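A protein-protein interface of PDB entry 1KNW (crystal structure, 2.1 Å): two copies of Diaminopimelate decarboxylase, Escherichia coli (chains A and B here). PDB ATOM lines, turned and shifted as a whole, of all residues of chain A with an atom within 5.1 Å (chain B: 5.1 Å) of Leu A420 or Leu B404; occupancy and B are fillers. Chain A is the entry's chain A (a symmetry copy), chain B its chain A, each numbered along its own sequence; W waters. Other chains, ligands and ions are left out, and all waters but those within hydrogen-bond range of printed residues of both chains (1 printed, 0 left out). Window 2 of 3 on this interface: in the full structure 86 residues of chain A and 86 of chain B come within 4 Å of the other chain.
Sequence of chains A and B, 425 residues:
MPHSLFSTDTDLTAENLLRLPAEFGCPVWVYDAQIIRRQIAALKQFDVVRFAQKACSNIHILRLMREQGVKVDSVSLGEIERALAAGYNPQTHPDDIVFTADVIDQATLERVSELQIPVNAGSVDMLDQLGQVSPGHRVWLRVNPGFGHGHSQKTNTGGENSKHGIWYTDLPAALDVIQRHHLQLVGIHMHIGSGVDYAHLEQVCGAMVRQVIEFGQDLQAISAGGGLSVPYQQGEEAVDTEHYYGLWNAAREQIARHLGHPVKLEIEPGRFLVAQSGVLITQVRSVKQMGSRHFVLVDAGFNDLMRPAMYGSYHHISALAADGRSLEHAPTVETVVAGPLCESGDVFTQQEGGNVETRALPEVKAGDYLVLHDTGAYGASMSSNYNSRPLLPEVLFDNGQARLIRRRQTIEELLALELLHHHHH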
ATOM      1  N   ALA A 416     -22.606 -27.804  -6.005  1.00  0.00           N
ATOM      2  CA  ALA A 416     -23.792 -26.969  -6.184  1.00  0.00           C
ATOM      3  C   ALA A 416     -23.540 -25.814  -7.139  1.00  0.00           C
ATOM      4  O   ALA A 416     -24.478 -25.315  -7.780  1.00  0.00           O
ATOM      5  CB  ALA A 416     -24.271 -26.429  -4.832  1.00  0.00           C
ATOM      6  N   LEU A 417     -22.290 -25.387  -7.288  1.00  0.00           N
ATOM      7  CA  LEU A 417     -21.942 -24.324  -8.223  1.00  0.00           C
ATOM      8  C   LEU A 417     -22.146 -24.775  -9.666  1.00  0.00           C
ATOM      9  O   LEU A 417     -22.419 -23.962 -10.551  1.00  0.00           O
ATOM     10  CB  LEU A 417     -20.489 -23.888  -8.022  1.00  0.00           C
ATOM     11  CG  LEU A 417     -20.071 -23.371  -6.656  1.00  0.00           C
ATOM     12  CD1 LEU A 417     -18.577 -23.037  -6.635  1.00  0.00           C
ATOM     13  CD2 LEU A 417     -20.878 -22.171  -6.214  1.00  0.00           C
ATOM     14  N   GLU A 418     -22.076 -26.077  -9.901  1.00  0.00           N
ATOM     15  CA  GLU A 418     -22.129 -26.658 -11.222  1.00  0.00           C
ATOM     16  C   GLU A 418     -23.465 -27.310 -11.540  1.00  0.00           C
ATOM     17  O   GLU A 418     -23.772 -27.586 -12.706  1.00  0.00           O
ATOM     18  CB  GLU A 418     -20.986 -27.697 -11.355  1.00  0.00           C
ATOM     19  CG  GLU A 418     -19.623 -27.085 -11.040  1.00  0.00           C
ATOM     20  CD  GLU A 418     -18.481 -28.064 -11.095  1.00  0.00           C
ATOM     21  OE1 GLU A 418     -18.633 -29.175 -11.645  1.00  0.00           O
ATOM     22  OE2 GLU A 418     -17.389 -27.735 -10.564  1.00  0.00           O
ATOM     23  N   LEU A 419     -24.254 -27.596 -10.518  1.00  0.00           N
ATOM     24  CA  LEU A 419     -25.580 -28.201 -10.708  1.00  0.00           C
ATOM     25  C   LEU A 419     -26.625 -27.078 -10.744  1.00  0.00           C
ATOM     26  O   LEU A 419     -26.926 -26.476  -9.713  1.00  0.00           O
ATOM     27  CB  LEU A 419     -25.886 -29.196  -9.602  1.00  0.00           C
ATOM     28  CG  LEU A 419     -24.963 -30.417  -9.499  1.00  0.00           C
ATOM     29  CD1 LEU A 419     -25.110 -31.087  -8.137  1.00  0.00           C
ATOM     30  CD2 LEU A 419     -25.247 -31.408 -10.621  1.00  0.00           C
ATOM     31  N   LEU A 420     -26.955 -26.631 -11.954  1.00  0.00           N
ATOM     32  CA  LEU A 420     -27.678 -25.386 -12.150  1.00  0.00           C
ATOM     33  C   LEU A 420     -29.173 -25.534 -12.261  1.00  0.00           C
ATOM     34  O   LEU A 420     -29.917 -24.536 -12.318  1.00  0.00           O
ATOM     35  CB  LEU A 420     -27.080 -24.636 -13.352  1.00  0.00           C
ATOM     36  CG  LEU A 420     -25.593 -24.261 -13.169  1.00  0.00           C
ATOM     37  CD1 LEU A 420     -24.982 -23.799 -14.467  1.00  0.00           C
ATOM     38  CD2 LEU A 420     -25.444 -23.227 -12.069  1.00  0.00           C
ATOM     39  N   HIS A 421     -29.676 -26.746 -12.239  1.00  0.00           N
ATOM     40  CA  HIS A 421     -31.081 -27.084 -12.180  1.00  0.00           C
ATOM     41  C   HIS A 421     -31.160 -28.628 -12.024  1.00  0.00           C
ATOM     42  O   HIS A 421     -31.405 -29.336 -12.987  1.00  0.00           O
ATOM     43  CB  HIS A 421     -31.899 -26.628 -13.357  1.00  0.00           C
ATOM     44  CG  HIS A 421     -33.386 -26.770 -13.188  1.00  0.00           C
ATOM     45  ND1 HIS A 421     -34.186 -25.748 -12.724  1.00  0.00           N
ATOM     46  CD2 HIS A 421     -34.210 -27.820 -13.414  1.00  0.00           C
ATOM     47  CE1 HIS A 421     -35.438 -26.161 -12.672  1.00  0.00           C
ATOM     48  NE2 HIS A 421     -35.480 -27.415 -13.086  1.00  0.00           N
ATOM     49  N   HIS A 422     -30.512 -29.074 -10.943  1.00  0.00           N
ATOM     50  CA  HIS A 422     -30.145 -30.454 -10.740  1.00  0.00           C
ATOM     51  C   HIS A 422     -28.798 -30.766 -11.398  1.00  0.00           C
ATOM     52  O   HIS A 422     -28.182 -29.832 -11.954  1.00  0.00           O
ATOM     53  CB  HIS A 422     -31.205 -31.430 -11.239  1.00  0.00           C
ATOM     54  CG  HIS A 422     -32.409 -31.503 -10.345  1.00  0.00           C
ATOM     55  ND1 HIS A 422     -33.511 -30.697 -10.532  1.00  0.00           N
ATOM     56  CD2 HIS A 422     -32.665 -32.250  -9.251  1.00  0.00           C
ATOM     57  CE1 HIS A 422     -34.408 -30.961  -9.598  1.00  0.00           C
ATOM     58  NE2 HIS A 422     -33.918 -31.900  -8.806  1.00  0.00           N
ATOM     59  N   PHE B  24     -21.835 -13.249 -18.829  1.00  0.00           N
ATOM     60  CA  PHE B  24     -21.592 -14.150 -17.723  1.00  0.00           C
ATOM     61  C   PHE B  24     -20.833 -13.566 -16.559  1.00  0.00           C
ATOM     62  O   PHE B  24     -20.625 -14.296 -15.558  1.00  0.00           O
ATOM     63  CB  PHE B  24     -20.841 -15.408 -18.236  1.00  0.00           C
ATOM     64  CG  PHE B  24     -21.647 -16.171 -19.256  1.00  0.00           C
ATOM     65  CD1 PHE B  24     -21.328 -16.103 -20.598  1.00  0.00           C
ATOM     66  CD2 PHE B  24     -22.735 -16.932 -18.868  1.00  0.00           C
ATOM     67  CE1 PHE B  24     -22.060 -16.816 -21.532  1.00  0.00           C
ATOM     68  CE2 PHE B  24     -23.480 -17.633 -19.798  1.00  0.00           C
ATOM     69  CZ  PHE B  24     -23.132 -17.578 -21.136  1.00  0.00           C
ATOM     70  N   PRO B 393     -16.949 -18.098 -12.443  1.00  0.00           N
ATOM     71  CA  PRO B 393     -17.848 -18.824 -13.313  1.00  0.00           C
ATOM     72  C   PRO B 393     -17.098 -19.524 -14.442  1.00  0.00           C
ATOM     73  O   PRO B 393     -16.035 -19.071 -14.867  1.00  0.00           O
ATOM     74  CB  PRO B 393     -18.753 -17.722 -13.895  1.00  0.00           C
ATOM     75  CG  PRO B 393     -17.923 -16.483 -13.829  1.00  0.00           C
ATOM     76  CD  PRO B 393     -17.130 -16.630 -12.535  1.00  0.00           C
ATOM     77  N   GLU B 394     -17.659 -20.623 -14.940  1.00  0.00           N
ATOM     78  CA  GLU B 394     -17.073 -21.344 -16.069  1.00  0.00           C
ATOM     79  C   GLU B 394     -18.128 -21.445 -17.187  1.00  0.00           C
ATOM     80  O   GLU B 394     -19.282 -21.713 -16.885  1.00  0.00           O
ATOM     81  CB  GLU B 394     -16.617 -22.747 -15.699  1.00  0.00           C
ATOM     82  CG  GLU B 394     -15.524 -22.789 -14.634  1.00  0.00           C
ATOM     83  CD  GLU B 394     -15.098 -24.215 -14.320  1.00  0.00           C
ATOM     84  OE1 GLU B 394     -15.771 -24.861 -13.502  1.00  0.00           O
ATOM     85  OE2 GLU B 394     -14.052 -24.647 -14.864  1.00  0.00           O
ATOM     86  N   VAL B 395     -17.701 -21.235 -18.408  1.00  0.00           N
ATOM     87  CA  VAL B 395     -18.552 -21.227 -19.581  1.00  0.00           C
ATOM     88  C   VAL B 395     -18.042 -22.228 -20.619  1.00  0.00           C
ATOM     89  O   VAL B 395     -16.842 -22.281 -20.876  1.00  0.00           O
ATOM     90  CB  VAL B 395     -18.506 -19.813 -20.255  1.00  0.00           C
ATOM     91  CG1 VAL B 395     -19.232 -19.817 -21.580  1.00  0.00           C
ATOM     92  CG2 VAL B 395     -19.075 -18.771 -19.313  1.00  0.00           C
ATOM     93  N   LEU B 396     -18.947 -22.989 -21.218  1.00  0.00           N
ATOM     94  CA  LEU B 396     -18.558 -23.976 -22.215  1.00  0.00           C
ATOM     95  C   LEU B 396     -19.099 -23.633 -23.600  1.00  0.00           C
ATOM     96  O   LEU B 396     -20.305 -23.516 -23.806  1.00  0.00           O
ATOM     97  CB  LEU B 396     -19.027 -25.376 -21.809  1.00  0.00           C
ATOM     98  CG  LEU B 396     -18.700 -26.526 -22.756  1.00  0.00           C
ATOM     99  CD1 LEU B 396     -17.193 -26.755 -22.866  1.00  0.00           C
ATOM    100  CD2 LEU B 396     -19.391 -27.806 -22.298  1.00  0.00           C
ATOM    101  N   ALA B 402     -22.346 -20.558 -26.265  1.00  0.00           N
ATOM    102  CA  ALA B 402     -21.755 -20.510 -24.934  1.00  0.00           C
ATOM    103  C   ALA B 402     -22.796 -20.737 -23.851  1.00  0.00           C
ATOM    104  O   ALA B 402     -23.856 -20.102 -23.847  1.00  0.00           O
ATOM    105  CB  ALA B 402     -21.058 -19.168 -24.714  1.00  0.00           C
ATOM    106  N   ARG B 403     -22.521 -21.677 -22.947  1.00  0.00           N
ATOM    107  CA  ARG B 403     -23.422 -21.962 -21.843  1.00  0.00           C
ATOM    108  C   ARG B 403     -22.664 -22.024 -20.506  1.00  0.00           C
ATOM    109  O   ARG B 403     -21.540 -22.500 -20.440  1.00  0.00           O
ATOM    110  CB  ARG B 403     -24.184 -23.261 -22.068  1.00  0.00           C
ATOM    111  CG  ARG B 403     -23.370 -24.519 -22.037  1.00  0.00           C
ATOM    112  CD  ARG B 403     -24.244 -25.777 -22.040  1.00  0.00           C
ATOM    113  NE  ARG B 403     -23.453 -26.941 -22.498  1.00  0.00           N
ATOM    114  CZ  ARG B 403     -23.408 -28.082 -21.817  1.00  0.00           C
ATOM    115  NH1 ARG B 403     -24.069 -28.191 -20.667  1.00  0.00           N
ATOM    116  NH2 ARG B 403     -22.684 -29.100 -22.263  1.00  0.00           N
ATOM    117  N   LEU B 404     -23.325 -21.585 -19.454  1.00  0.00           N
ATOM    118  CA  LEU B 404     -22.766 -21.595 -18.103  1.00  0.00           C
ATOM    119  C   LEU B 404     -22.650 -23.048 -17.607  1.00  0.00           C
ATOM    120  O   LEU B 404     -23.648 -23.755 -17.600  1.00  0.00           O
ATOM    121  CB  LEU B 404     -23.735 -20.875 -17.162  1.00  0.00           C
ATOM    122  CG  LEU B 404     -23.269 -19.916 -16.119  1.00  0.00           C
ATOM    123  CD1 LEU B 404     -23.936 -20.178 -14.769  1.00  0.00           C
ATOM    124  CD2 LEU B 404     -21.783 -19.756 -15.981  1.00  0.00           C
ATOM    125  N   ILE B 405     -21.476 -23.430 -17.127  1.00  0.00           N
ATOM    126  CA  ILE B 405     -21.288 -24.760 -16.565  1.00  0.00           C
ATOM    127  C   ILE B 405     -20.818 -24.684 -15.120  1.00  0.00           C
ATOM    128  O   ILE B 405     -20.731 -25.703 -14.424  1.00  0.00           O
ATOM    129  CB  ILE B 405     -20.363 -25.643 -17.396  1.00  0.00           C
ATOM    130  CG1 ILE B 405     -19.042 -24.943 -17.705  1.00  0.00           C
ATOM    131  CG2 ILE B 405     -21.050 -26.071 -18.695  1.00  0.00           C
ATOM    132  CD1 ILE B 405     -17.884 -25.881 -17.973  1.00  0.00           C
ATOM    133  N   ARG B 406     -20.560 -23.471 -14.636  1.00  0.00           N
ATOM    134  CA  ARG B 406     -20.359 -23.214 -13.225  1.00  0.00           C
ATOM    135  C   ARG B 406     -20.690 -21.748 -12.921  1.00  0.00           C
ATOM    136  O   ARG B 406     -20.205 -20.872 -13.632  1.00  0.00           O
ATOM    137  CB  ARG B 406     -18.926 -23.494 -12.742  1.00  0.00           C
ATOM    138  CG  ARG B 406     -18.778 -23.272 -11.228  1.00  0.00           C
ATOM    139  CD  ARG B 406     -17.423 -23.780 -10.715  1.00  0.00           C
ATOM    140  NE  ARG B 406     -16.387 -22.759 -10.859  1.00  0.00           N
ATOM    141  CZ  ARG B 406     -15.095 -22.927 -10.624  1.00  0.00           C
ATOM    142  NH1 ARG B 406     -14.253 -21.922 -10.813  1.00  0.00           N
ATOM    143  NH2 ARG B 406     -14.614 -24.107 -10.220  1.00  0.00           N
ATOM    144  N   ARG B 407     -21.539 -21.522 -11.927  1.00  0.00           N
ATOM    145  CA  ARG B 407     -21.868 -20.145 -11.554  1.00  0.00           C
ATOM    146  C   ARG B 407     -20.813 -19.614 -10.575  1.00  0.00           C
ATOM    147  O   ARG B 407     -20.056 -20.388  -9.995  1.00  0.00           O
ATOM    148  CB  ARG B 407     -23.248 -20.046 -10.925  1.00  0.00           C
ATOM    149  CG  ARG B 407     -23.402 -20.746  -9.608  1.00  0.00           C
ATOM    150  CD  ARG B 407     -24.719 -20.357  -8.907  1.00  0.00           C
ATOM    151  NE  ARG B 407     -24.662 -20.793  -7.521  1.00  0.00           N
ATOM    152  CZ  ARG B 407     -25.209 -21.865  -6.998  1.00  0.00           C
ATOM    153  NH1 ARG B 407     -25.997 -22.656  -7.721  1.00  0.00           N
ATOM    154  NH2 ARG B 407     -25.002 -22.139  -5.705  1.00  0.00           N
HETATM  155  O   HOH W   1     -15.139 -26.747 -11.702  1.00  0.00           O
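The side-chain carboxylate (OE1) of Glu B394 is in salt-bridge range of the guanidinium group (NE) of Arg B406, 3.4 Å away. The backbone NH (N) of Ile B405 lies within hydrogen-bond range of the backbone carbonyl oxygen (O) of Glu B394 (2.8 Å).
Water W1 lies within hydrogen-bond range of the side-chain carboxylate of Glu B394 (2.7 Å), the side-chain carboxylate of Glu A418 (2.7 Å) and the guanidinium group of Arg B406 (3.1 Å).
Of the 11 printed residues of chain B, 4 touch a printed residue of chain A. Hydrophobic or aromatic side chains of chain B that line the printed part of chain A: Leu B404. Along chain B the printed residues that touch a printed residue of chain A span positions 404 to 407. Hydrophobic or aromatic side chains of chain A within 4 Å of the printed part of chain B: Leu A417 and Leu A420.
Among the printed residues, merely in contact across the chains: Leu A420 with Leu B404 (3.4 Å), Leu A417 with Arg B406 (3.5 Å), Glu A418 with Ile B405 (3.6 Å) and Glu A418 with Arg B406 (3.9 Å).
The backbone carbonyl oxygen of Leu A417 lies within hydrogen-bond range of the backbone NH of Arg B407, 2.9 Å away. The guanidinium group of Arg B407 sits at hydrogen-bond distance from the backbone carbonyl oxygen of Ala A416 (3.1 Å).
No position is printed for both chains. Of the 6 pairs that touch across the chains among the printed residues, none has its exchanged pair printed and touching as well.
Of the printed residues of chain B, Ala A416 touches Arg B407. Of chain B, only Leu B404 comes within 4 Å of Leu A420. Val B395 touches none of the printed residues of chain A. Printed residues of chain A within 4 Å of Leu B404: Leu A420. Of the printed residues of chain A, Ile B405 touches Glu A418 (3.6 Å). Printed residues of chain A within 4 Å of Arg B406: Leu A417 (3.5 Å) and Glu A418 (3.9 Å). Printed residues of chain A within 4 Å of Arg B407: Ala A416 (3.1 Å) and Leu A417 (2.9 Å). The nearest residue of chain B that does not touch Leu A420 is Arg B407 (4.03 Å). The nearest printed residue of chain A that does not touch Leu B404 is Leu A417 (5.9 Å). The nearest printed residue of chain B that does not touch Leu A417 is Ile B405 (4.6 Å).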
